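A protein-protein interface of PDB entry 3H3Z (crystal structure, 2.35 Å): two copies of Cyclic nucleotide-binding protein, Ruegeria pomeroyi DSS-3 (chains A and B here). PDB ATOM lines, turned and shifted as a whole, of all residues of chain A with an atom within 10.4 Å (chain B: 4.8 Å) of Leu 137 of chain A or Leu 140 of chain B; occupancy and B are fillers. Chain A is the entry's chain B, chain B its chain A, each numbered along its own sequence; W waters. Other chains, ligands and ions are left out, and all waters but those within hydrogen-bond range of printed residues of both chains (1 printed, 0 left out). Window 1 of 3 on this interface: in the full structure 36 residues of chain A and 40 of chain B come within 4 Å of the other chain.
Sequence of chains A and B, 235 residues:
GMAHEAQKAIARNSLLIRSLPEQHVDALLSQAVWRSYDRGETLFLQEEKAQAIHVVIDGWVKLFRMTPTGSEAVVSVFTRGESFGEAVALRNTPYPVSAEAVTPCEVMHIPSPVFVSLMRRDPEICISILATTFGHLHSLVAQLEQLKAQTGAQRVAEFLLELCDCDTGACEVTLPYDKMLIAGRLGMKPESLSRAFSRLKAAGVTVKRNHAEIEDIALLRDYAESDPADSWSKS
The side-chain hydroxyl (OG1) of Thr 133 of chain B is in hydrogen-bond range of the side-chain hydroxyl (OG1) of Thr 133 of chain A (3.1 Å).
O of Ile 129 of chain A sits close to OG1 of Thr 133 of chain A (3.4 Å).
The side-chain hydroxyl (OG) of Ser 19 of chain A is in hydrogen-bond range of the backbone carbonyl oxygen (O) of Leu 15 of chain A, 2.5 Å away.
The backbone carbonyl oxygen of Leu 130 of chain A is in hydrogen-bond range of the side-chain hydroxyl of Thr 133 of chain A, at 3.1 Å.
Among the printed residues, merely in contact across the chains: Leu 15 of chain A with His 138 of chain B, Leu 144 of chain A with Leu 140 of chain B, His 138 of chain A with Leu 15 of chain B, Val 141 of chain A with Leu 140 of chain B, His 136 of chain A with Leu 137 of chain B, Leu 140 of chain A with Leu 144 of chain B, Leu 130 of chain A with Thr 133 of chain B, Leu 140 of chain A with Leu 137 of chain B, Leu 137 of chain A with Leu 140 of chain B, Leu 137 of chain A with His 136 of chain B, Leu 144 of chain A with Leu 144 of chain B, Leu 137 of chain A with Leu 137 of chain B, Leu 144 of chain A with Gln 143 of chain B, Leu 137 of chain A with Thr 133 of chain B, Leu 140 of chain A with Val 141 of chain B, Leu 137 of chain A with Leu 15 of chain B and Leu 140 of chain A with Leu 140 of chain B.
Of the printed residues of chain B, Leu 137 of chain A touches Leu 15 (3.95 Å), Thr 133 (3.8 Å), His 136 (3.6 Å), Leu 137 (3.7 Å) and Leu 140 (3.6 Å).
Thr 133 of chain B touches just these residues of chain A: Leu 130 (3.6 Å), Thr 133 (3.1 Å) and Leu 137 (3.8 Å).
No residue of chain A comes within 4 Å of Ser 139 of chain B.
Of chain A, only Leu 140 comes within 4 Å of Val 141 of chain B.
Of chain A, only Leu 144 (3.7 Å) comes within 4 Å of Gln 143 of chain B.
Of the printed residues of chain B, Thr 133 of chain A touches Thr 133.
Printed residues of chain A within 4 Å of His 136 of chain B: Leu 137 (3.6 Å).
Printed residues of chain B within 4 Å of His 138 of chain A: Leu 15.
Of the printed residues of chain B, Val 141 of chain A touches Leu 140.
Of the printed residues of chain B, Leu 15 of chain A touches His 138 (3.4 Å).
Glu 145 of chain A touches none of the printed residues of chain B.
Gln 143 of chain A touches none of the printed residues of chain B.
The nearest printed residue of chain A that does not touch Leu 140 of chain B is His 136 of chain A (5.9 Å).
Of the 11 printed residues of chain B, 9 touch a printed residue of chain A.
Printed residues of chain B that touch a printed residue of chain A: Leu 15, Thr 133, His 136, Leu 137, His 138, Leu 140, Val 141, Gln 143 and Leu 144.
Hydrophobic or aromatic side chains of chain B within 4 Å of the printed part of chain A: Leu 15, His 136, Leu 137, His 138, Leu 140, Val 141 and Leu 144.
Along chain B the printed residues that touch a printed residue of chain A span positions 15 to 144.
Of the 21 printed residues of chain A, 9 touch a printed residue of chain B.
Printed residues of chain A that touch a printed residue of chain B: Leu 15, Leu 130, Thr 133, His 136, Leu 137, His 138, Leu 140, Val 141 and Leu 144.
Hydrophobic or aromatic side chains of chain A within 4 Å of the printed part of chain B: Leu 15, Leu 130, His 136, Leu 137, His 138, Leu 140, Val 141 and Leu 144.
Among the printed residues, 18 pairs touch across the chains.
Among the printed residues, no Asp or Glu carboxylate lies within 4 Å of a Lys or Arg side-chain nitrogen of the other chain.
Leu 15 of chain A touches His 138 of chain B, and with the chains exchanged His 138 of chain A touches Leu 15 of chain B.
His 136 of chain A touches Leu 137 of chain B, and with the chains exchanged Leu 137 of chain A touches His 136 of chain B.
Leu 137 of chain A touches its own counterpart, Leu 137 of chain B.
Leu 144 of chain B touches its own counterpart, Leu 144 of chain A.
Water W1 lies within hydrogen-bond range of O of Arg 185 of chain A (2.6 Å) and O of Ala 142 of chain B (3.5 Å).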
ATOM      1  N   LEU A  15      21.973 -12.615  19.464  1.00  0.00           N
ATOM      2  CA  LEU A  15      21.130 -11.599  18.898  1.00  0.00           C
ATOM      3  C   LEU A  15      21.574 -11.256  17.500  1.00  0.00           C
ATOM      4  O   LEU A  15      20.758 -11.138  16.594  1.00  0.00           O
ATOM      5  CB  LEU A  15      21.243 -10.335  19.767  1.00  0.00           C
ATOM      6  CG  LEU A  15      20.163  -9.267  19.800  1.00  0.00           C
ATOM      7  CD1 LEU A  15      19.010  -9.735  20.710  1.00  0.00           C
ATOM      8  CD2 LEU A  15      20.716  -7.954  20.308  1.00  0.00           C
ATOM      9  N   SER A  19      19.474 -12.491  14.046  1.00  0.00           N
ATOM     10  CA  SER A  19      18.861 -11.459  13.221  1.00  0.00           C
ATOM     11  C   SER A  19      19.224 -11.491  11.725  1.00  0.00           C
ATOM     12  O   SER A  19      18.623 -10.771  10.916  1.00  0.00           O
ATOM     13  CB  SER A  19      19.283 -10.124  13.808  1.00  0.00           C
ATOM     14  OG  SER A  19      19.001 -10.125  15.217  1.00  0.00           O
ATOM     15  N   ILE A 129      17.318  -7.688   7.589  1.00  0.00           N
ATOM     16  CA  ILE A 129      17.765  -7.783   8.982  1.00  0.00           C
ATOM     17  C   ILE A 129      16.894  -6.903   9.847  1.00  0.00           C
ATOM     18  O   ILE A 129      16.522  -7.277  10.937  1.00  0.00           O
ATOM     19  CB  ILE A 129      19.249  -7.405   9.136  1.00  0.00           C
ATOM     20  CG1 ILE A 129      20.152  -8.414   8.395  1.00  0.00           C
ATOM     21  CG2 ILE A 129      19.626  -7.382  10.589  1.00  0.00           C
ATOM     22  CD1 ILE A 129      21.589  -7.909   8.063  1.00  0.00           C
ATOM     23  N   LEU A 130      16.548  -5.742   9.317  1.00  0.00           N
ATOM     24  CA  LEU A 130      15.744  -4.744  10.013  1.00  0.00           C
ATOM     25  C   LEU A 130      14.298  -5.225  10.226  1.00  0.00           C
ATOM     26  O   LEU A 130      13.655  -4.911  11.255  1.00  0.00           O
ATOM     27  CB  LEU A 130      15.812  -3.442   9.229  1.00  0.00           C
ATOM     28  CG  LEU A 130      15.206  -2.151   9.764  1.00  0.00           C
ATOM     29  CD1 LEU A 130      15.654  -1.833  11.240  1.00  0.00           C
ATOM     30  CD2 LEU A 130      15.527  -0.993   8.766  1.00  0.00           C
ATOM     31  N   ALA A 131      13.789  -5.992   9.274  1.00  0.00           N
ATOM     32  CA  ALA A 131      12.465  -6.576   9.394  1.00  0.00           C
ATOM     33  C   ALA A 131      12.475  -7.494  10.621  1.00  0.00           C
ATOM     34  O   ALA A 131      11.568  -7.477  11.431  1.00  0.00           O
ATOM     35  CB  ALA A 131      12.079  -7.348   8.114  1.00  0.00           C
ATOM     36  N   THR A 132      13.543  -8.260  10.776  1.00  0.00           N
ATOM     37  CA  THR A 132      13.665  -9.211  11.873  1.00  0.00           C
ATOM     38  C   THR A 132      13.868  -8.520  13.207  1.00  0.00           C
ATOM     39  O   THR A 132      13.282  -8.910  14.225  1.00  0.00           O
ATOM     40  CB  THR A 132      14.807 -10.151  11.560  1.00  0.00           C
ATOM     41  OG1 THR A 132      14.520 -10.736  10.294  1.00  0.00           O
ATOM     42  CG2 THR A 132      15.029 -11.286  12.645  1.00  0.00           C
ATOM     43  N   THR A 133      14.650  -7.458  13.202  1.00  0.00           N
ATOM     44  CA  THR A 133      14.885  -6.719  14.429  1.00  0.00           C
ATOM     45  C   THR A 133      13.634  -5.941  14.860  1.00  0.00           C
ATOM     46  O   THR A 133      13.438  -5.735  16.058  1.00  0.00           O
ATOM     47  CB  THR A 133      16.152  -5.826  14.315  1.00  0.00           C
ATOM     48  OG1 THR A 133      15.985  -4.855  13.301  1.00  0.00           O
ATOM     49  CG2 THR A 133      17.319  -6.667  13.939  1.00  0.00           C
ATOM     50  N   PHE A 134      12.783  -5.536  13.922  1.00  0.00           N
ATOM     51  CA  PHE A 134      11.502  -4.892  14.279  1.00  0.00           C
ATOM     52  C   PHE A 134      10.501  -5.874  14.889  1.00  0.00           C
ATOM     53  O   PHE A 134       9.782  -5.548  15.854  1.00  0.00           O
ATOM     54  CB  PHE A 134      10.819  -4.207  13.082  1.00  0.00           C
ATOM     55  CG  PHE A 134      11.265  -2.773  12.851  1.00  0.00           C
ATOM     56  CD1 PHE A 134      10.978  -1.785  13.791  1.00  0.00           C
ATOM     57  CD2 PHE A 134      11.934  -2.403  11.679  1.00  0.00           C
ATOM     58  CE1 PHE A 134      11.356  -0.468  13.589  1.00  0.00           C
ATOM     59  CE2 PHE A 134      12.310  -1.082  11.468  1.00  0.00           C
ATOM     60  CZ  PHE A 134      12.026  -0.116  12.412  1.00  0.00           C
ATOM     61  N   GLY A 135      10.413  -7.056  14.295  1.00  0.00           N
ATOM     62  CA  GLY A 135       9.529  -8.084  14.801  1.00  0.00           C
ATOM     63  C   GLY A 135       9.944  -8.502  16.207  1.00  0.00           C
ATOM     64  O   GLY A 135       9.096  -8.696  17.071  1.00  0.00           O
ATOM     65  N   HIS A 136      11.246  -8.564  16.458  1.00  0.00           N
ATOM     66  CA  HIS A 136      11.729  -8.954  17.764  1.00  0.00           C
ATOM     67  C   HIS A 136      11.464  -7.816  18.741  1.00  0.00           C
ATOM     68  O   HIS A 136      11.025  -8.038  19.856  1.00  0.00           O
ATOM     69  CB  HIS A 136      13.201  -9.366  17.696  1.00  0.00           C
ATOM     70  CG  HIS A 136      13.686 -10.085  18.916  1.00  0.00           C
ATOM     71  ND1 HIS A 136      15.003 -10.074  19.303  1.00  0.00           N
ATOM     72  CD2 HIS A 136      13.028 -10.810  19.856  1.00  0.00           C
ATOM     73  CE1 HIS A 136      15.147 -10.782  20.408  1.00  0.00           C
ATOM     74  NE2 HIS A 136      13.960 -11.231  20.772  1.00  0.00           N
ATOM     75  N   LEU A 137      11.666  -6.591  18.299  1.00  0.00           N
ATOM     76  CA  LEU A 137      11.356  -5.445  19.167  1.00  0.00           C
ATOM     77  C   LEU A 137       9.896  -5.484  19.626  1.00  0.00           C
ATOM     78  O   LEU A 137       9.592  -5.293  20.808  1.00  0.00           O
ATOM     79  CB  LEU A 137      11.636  -4.101  18.478  1.00  0.00           C
ATOM     80  CG  LEU A 137      13.031  -3.504  18.559  1.00  0.00           C
ATOM     81  CD1 LEU A 137      13.231  -2.409  17.469  1.00  0.00           C
ATOM     82  CD2 LEU A 137      13.291  -2.981  19.980  1.00  0.00           C
ATOM     83  N   HIS A 138       8.990  -5.706  18.682  1.00  0.00           N
ATOM     84  CA  HIS A 138       7.566  -5.844  19.022  1.00  0.00           C
ATOM     85  C   HIS A 138       7.319  -6.962  19.981  1.00  0.00           C
ATOM     86  O   HIS A 138       6.555  -6.818  20.918  1.00  0.00           O
ATOM     87  CB  HIS A 138       6.723  -6.090  17.781  1.00  0.00           C
ATOM     88  CG  HIS A 138       6.361  -4.829  17.087  1.00  0.00           C
ATOM     89  ND1 HIS A 138       5.500  -3.907  17.656  1.00  0.00           N
ATOM     90  CD2 HIS A 138       6.764  -4.306  15.902  1.00  0.00           C
ATOM     91  CE1 HIS A 138       5.360  -2.891  16.821  1.00  0.00           C
ATOM     92  NE2 HIS A 138       6.112  -3.108  15.752  1.00  0.00           N
ATOM     93  N   SER A 139       7.965  -8.083  19.759  1.00  0.00           N
ATOM     94  CA  SER A 139       7.780  -9.218  20.681  1.00  0.00           C
ATOM     95  C   SER A 139       8.258  -8.889  22.126  1.00  0.00           C
ATOM     96  O   SER A 139       7.568  -9.181  23.116  1.00  0.00           O
ATOM     97  CB  SER A 139       8.491 -10.442  20.100  1.00  0.00           C
ATOM     98  OG  SER A 139       8.602 -11.440  21.086  1.00  0.00           O
ATOM     99  N   LEU A 140       9.413  -8.248  22.244  1.00  0.00           N
ATOM    100  CA  LEU A 140       9.939  -7.856  23.556  1.00  0.00           C
ATOM    101  C   LEU A 140       9.040  -6.820  24.265  1.00  0.00           C
ATOM    102  O   LEU A 140       8.776  -6.919  25.476  1.00  0.00           O
ATOM    103  CB  LEU A 140      11.366  -7.303  23.422  1.00  0.00           C
ATOM    104  CG  LEU A 140      12.439  -8.309  22.973  1.00  0.00           C
ATOM    105  CD1 LEU A 140      13.780  -7.613  22.764  1.00  0.00           C
ATOM    106  CD2 LEU A 140      12.579  -9.491  23.977  1.00  0.00           C
ATOM    107  N   VAL A 141       8.557  -5.837  23.509  1.00  0.00           N
ATOM    108  CA  VAL A 141       7.625  -4.856  24.046  1.00  0.00           C
ATOM    109  C   VAL A 141       6.323  -5.527  24.530  1.00  0.00           C
ATOM    110  O   VAL A 141       5.837  -5.214  25.616  1.00  0.00           O
ATOM    111  CB  VAL A 141       7.300  -3.730  23.009  1.00  0.00           C
ATOM    112  CG1 VAL A 141       6.120  -2.900  23.485  1.00  0.00           C
ATOM    113  CG2 VAL A 141       8.534  -2.841  22.753  1.00  0.00           C
ATOM    114  N   ALA A 142       5.785  -6.469  23.750  1.00  0.00           N
ATOM    115  CA  ALA A 142       4.583  -7.209  24.135  1.00  0.00           C
ATOM    116  C   ALA A 142       4.851  -7.977  25.396  1.00  0.00           C
ATOM    117  O   ALA A 142       4.046  -7.993  26.331  1.00  0.00           O
ATOM    118  CB  ALA A 142       4.153  -8.157  23.018  1.00  0.00           C
ATOM    119  N   GLN A 143       6.011  -8.608  25.453  1.00  0.00           N
ATOM    120  CA  GLN A 143       6.360  -9.430  26.622  1.00  0.00           C
ATOM    121  C   GLN A 143       6.545  -8.540  27.888  1.00  0.00           C
ATOM    122  O   GLN A 143       6.168  -8.935  28.997  1.00  0.00           O
ATOM    123  CB  GLN A 143       7.589 -10.278  26.281  1.00  0.00           C
ATOM    124  CG  GLN A 143       7.675 -11.604  26.962  1.00  0.00           C
ATOM    125  CD  GLN A 143       8.917 -12.429  26.577  1.00  0.00           C
ATOM    126  OE1 GLN A 143       9.463 -13.173  27.415  1.00  0.00           O
ATOM    127  NE2 GLN A 143       9.369 -12.304  25.326  1.00  0.00           N
ATOM    128  N   LEU A 144       7.079  -7.325  27.727  1.00  0.00           N
ATOM    129  CA  LEU A 144       7.225  -6.413  28.869  1.00  0.00           C
ATOM    130  C   LEU A 144       5.896  -5.903  29.423  1.00  0.00           C
ATOM    131  O   LEU A 144       5.853  -5.395  30.519  1.00  0.00           O
ATOM    132  CB  LEU A 144       8.099  -5.201  28.520  1.00  0.00           C
ATOM    133  CG  LEU A 144       9.605  -5.378  28.652  1.00  0.00           C
ATOM    134  CD1 LEU A 144      10.354  -4.209  27.938  1.00  0.00           C
ATOM    135  CD2 LEU A 144       9.997  -5.525  30.137  1.00  0.00           C
ATOM    136  N   GLU A 145       4.819  -5.988  28.664  1.00  0.00           N
ATOM    137  CA  GLU A 145       3.508  -5.576  29.187  1.00  0.00           C
ATOM    138  C   GLU A 145       2.772  -6.655  29.941  1.00  0.00           C
ATOM    139  O   GLU A 145       1.801  -6.382  30.615  1.00  0.00           O
ATOM    140  CB  GLU A 145       2.608  -5.112  28.048  1.00  0.00           C
ATOM    141  CG  GLU A 145       3.121  -3.880  27.427  1.00  0.00           C
ATOM    142  CD  GLU A 145       2.052  -3.036  26.898  1.00  0.00           C
ATOM    143  OE1 GLU A 145       1.254  -2.482  27.724  1.00  0.00           O
ATOM    144  OE2 GLU A 145       2.053  -2.911  25.649  1.00  0.00           O
ATOM    145  N   LYS A 148       4.349 -10.112  35.362  1.00  0.00           N
ATOM    146  CA  LYS A 148       5.317 -11.077  35.876  1.00  0.00           C
ATOM    147  C   LYS A 148       4.873 -11.405  37.286  1.00  0.00           C
ATOM    148  O   LYS A 148       4.519 -10.512  38.041  1.00  0.00           O
ATOM    149  CB  LYS A 148       6.766 -10.559  35.863  1.00  0.00           C
ATOM    150  CG  LYS A 148       7.778 -11.719  36.022  1.00  0.00           C
ATOM    151  CD  LYS A 148       9.129 -11.558  35.288  1.00  0.00           C
ATOM    152  CE  LYS A 148       9.835 -12.928  35.288  1.00  0.00           C
ATOM    153  NZ  LYS A 148      11.129 -13.080  34.568  1.00  0.00           N
ATOM    154  N   ARG A 185      22.695  -7.757  36.964  1.00  0.00           N
ATOM    155  CA  ARG A 185      22.036  -8.211  35.759  1.00  0.00           C
ATOM    156  C   ARG A 185      20.556  -8.557  35.994  1.00  0.00           C
ATOM    157  O   ARG A 185      19.683  -8.215  35.174  1.00  0.00           O
ATOM    158  CB  ARG A 185      22.757  -9.429  35.217  1.00  0.00           C
ATOM    159  CG  ARG A 185      22.154  -9.892  33.947  1.00  0.00           C
ATOM    160  CD  ARG A 185      23.139 -10.699  33.195  1.00  0.00           C
ATOM    161  NE  ARG A 185      22.472 -11.410  32.126  1.00  0.00           N
ATOM    162  CZ  ARG A 185      23.076 -11.979  31.086  1.00  0.00           C
ATOM    163  NH1 ARG A 185      24.394 -11.936  30.920  1.00  0.00           N
ATOM    164  NH2 ARG A 185      22.321 -12.594  30.193  1.00  0.00           N
ATOM    165  N   LEU B  15       7.255   3.121  17.795  1.00  0.00           N
ATOM    166  CA  LEU B  15       8.472   2.373  17.524  1.00  0.00           C
ATOM    167  C   LEU B  15       9.077   2.714  16.145  1.00  0.00           C
ATOM    168  O   LEU B  15      10.273   2.831  15.990  1.00  0.00           O
ATOM    169  CB  LEU B  15       8.131   0.894  17.570  1.00  0.00           C
ATOM    170  CG  LEU B  15       9.188  -0.190  17.501  1.00  0.00           C
ATOM    171  CD1 LEU B  15      10.346   0.099  18.480  1.00  0.00           C
ATOM    172  CD2 LEU B  15       8.502  -1.516  17.808  1.00  0.00           C
ATOM    173  N   THR B 133      17.963   0.044  16.323  1.00  0.00           N
ATOM    174  CA  THR B 133      17.122  -1.051  16.738  1.00  0.00           C
ATOM    175  C   THR B 133      17.916  -2.060  17.564  1.00  0.00           C
ATOM    176  O   THR B 133      17.338  -2.648  18.488  1.00  0.00           O
ATOM    177  CB  THR B 133      16.418  -1.746  15.542  1.00  0.00           C
ATOM    178  OG1 THR B 133      17.377  -2.483  14.780  1.00  0.00           O
ATOM    179  CG2 THR B 133      15.732  -0.713  14.670  1.00  0.00           C
ATOM    180  N   HIS B 136      18.108  -0.621  21.075  1.00  0.00           N
ATOM    181  CA  HIS B 136      16.790  -0.763  21.652  1.00  0.00           C
ATOM    182  C   HIS B 136      16.542  -2.218  22.098  1.00  0.00           C
ATOM    183  O   HIS B 136      15.951  -2.453  23.148  1.00  0.00           O
ATOM    184  CB  HIS B 136      15.691  -0.321  20.660  1.00  0.00           C
ATOM    185  CG  HIS B 136      15.584   1.171  20.435  1.00  0.00           C
ATOM    186  ND1 HIS B 136      15.877   2.107  21.406  1.00  0.00           N
ATOM    187  CD2 HIS B 136      15.078   1.874  19.384  1.00  0.00           C
ATOM    188  CE1 HIS B 136      15.638   3.321  20.938  1.00  0.00           C
ATOM    189  NE2 HIS B 136      15.142   3.209  19.716  1.00  0.00           N
ATOM    190  N   LEU B 137      16.999  -3.187  21.311  1.00  0.00           N
ATOM    191  CA  LEU B 137      16.849  -4.602  21.653  1.00  0.00           C
ATOM    192  C   LEU B 137      17.594  -5.002  22.946  1.00  0.00           C
ATOM    193  O   LEU B 137      17.058  -5.717  23.755  1.00  0.00           O
ATOM    194  CB  LEU B 137      17.337  -5.543  20.528  1.00  0.00           C
ATOM    195  CG  LEU B 137      16.502  -5.802  19.268  1.00  0.00           C
ATOM    196  CD1 LEU B 137      17.327  -6.598  18.264  1.00  0.00           C
ATOM    197  CD2 LEU B 137      15.168  -6.517  19.583  1.00  0.00           C
ATOM    198  N   HIS B 138      18.871  -4.647  23.039  1.00  0.00           N
ATOM    199  CA  HIS B 138      19.667  -4.908  24.221  1.00  0.00           C
ATOM    200  C   HIS B 138      19.012  -4.250  25.455  1.00  0.00           C
ATOM    201  O   HIS B 138      18.958  -4.826  26.537  1.00  0.00           O
ATOM    202  CB  HIS B 138      21.082  -4.354  24.044  1.00  0.00           C
ATOM    203  CG  HIS B 138      21.964  -5.186  23.183  1.00  0.00           C
ATOM    204  ND1 HIS B 138      22.466  -6.393  23.599  1.00  0.00           N
ATOM    205  CD2 HIS B 138      22.475  -4.972  21.946  1.00  0.00           C
ATOM    206  CE1 HIS B 138      23.233  -6.900  22.653  1.00  0.00           C
ATOM    207  NE2 HIS B 138      23.263  -6.053  21.640  1.00  0.00           N
ATOM    208  N   SER B 139      18.509  -3.041  25.271  1.00  0.00           N
ATOM    209  CA  SER B 139      17.838  -2.319  26.335  1.00  0.00           C
ATOM    210  C   SER B 139      16.577  -3.010  26.835  1.00  0.00           C
ATOM    211  O   SER B 139      16.365  -3.050  28.058  1.00  0.00           O
ATOM    212  CB  SER B 139      17.519  -0.917  25.846  1.00  0.00           C
ATOM    213  OG  SER B 139      16.585  -0.286  26.683  1.00  0.00           O
ATOM    214  N   LEU B 140      15.733  -3.527  25.919  1.00  0.00           N
ATOM    215  CA  LEU B 140      14.512  -4.264  26.311  1.00  0.00           C
ATOM    216  C   LEU B 140      14.845  -5.614  26.927  1.00  0.00           C
ATOM    217  O   LEU B 140      14.234  -6.008  27.902  1.00  0.00           O
ATOM    218  CB  LEU B 140      13.544  -4.432  25.141  1.00  0.00           C
ATOM    219  CG  LEU B 140      12.924  -3.119  24.557  1.00  0.00           C
ATOM    220  CD1 LEU B 140      12.005  -3.383  23.367  1.00  0.00           C
ATOM    221  CD2 LEU B 140      12.146  -2.319  25.561  1.00  0.00           C
ATOM    222  N   VAL B 141      15.808  -6.335  26.373  1.00  0.00           N
ATOM    223  CA  VAL B 141      16.256  -7.578  27.002  1.00  0.00           C
ATOM    224  C   VAL B 141      16.696  -7.310  28.470  1.00  0.00           C
ATOM    225  O   VAL B 141      16.314  -8.041  29.363  1.00  0.00           O
ATOM    226  CB  VAL B 141      17.382  -8.274  26.208  1.00  0.00           C
ATOM    227  CG1 VAL B 141      18.014  -9.413  27.014  1.00  0.00           C
ATOM    228  CG2 VAL B 141      16.862  -8.836  24.856  1.00  0.00           C
ATOM    229  N   ALA B 142      17.455  -6.245  28.708  1.00  0.00           N
ATOM    230  CA  ALA B 142      17.914  -5.889  30.067  1.00  0.00           C
ATOM    231  C   ALA B 142      16.731  -5.536  30.956  1.00  0.00           C
ATOM    232  O   ALA B 142      16.707  -5.877  32.130  1.00  0.00           O
ATOM    233  CB  ALA B 142      18.989  -4.743  30.034  1.00  0.00           C
ATOM    234  N   GLN B 143      15.722  -4.882  30.400  1.00  0.00           N
ATOM    235  CA  GLN B 143      14.521  -4.614  31.198  1.00  0.00           C
ATOM    236  C   GLN B 143      13.810  -5.911  31.568  1.00  0.00           C
ATOM    237  O   GLN B 143      13.335  -6.029  32.688  1.00  0.00           O
ATOM    238  CB  GLN B 143      13.560  -3.709  30.493  1.00  0.00           C
ATOM    239  CG  GLN B 143      14.116  -2.351  30.303  1.00  0.00           C
ATOM    240  CD  GLN B 143      13.188  -1.444  29.512  1.00  0.00           C
ATOM    241  OE1 GLN B 143      13.616  -0.765  28.562  1.00  0.00           O
ATOM    242  NE2 GLN B 143      11.915  -1.434  29.892  1.00  0.00           N
ATOM    243  N   LEU B 144      13.781  -6.875  30.642  1.00  0.00           N
ATOM    244  CA  LEU B 144      13.133  -8.160  30.897  1.00  0.00           C
ATOM    245  C   LEU B 144      13.908  -8.905  31.925  1.00  0.00           C
ATOM    246  O   LEU B 144      13.344  -9.503  32.780  1.00  0.00           O
ATOM    247  CB  LEU B 144      12.974  -9.040  29.635  1.00  0.00           C
ATOM    248  CG  LEU B 144      11.724  -8.790  28.777  1.00  0.00           C
ATOM    249  CD1 LEU B 144      11.764  -9.588  27.477  1.00  0.00           C
ATOM    250  CD2 LEU B 144      10.473  -9.160  29.547  1.00  0.00           C
HETATM  251  O   HOH W   1      19.967  -6.826  32.959  1.00  0.00           O
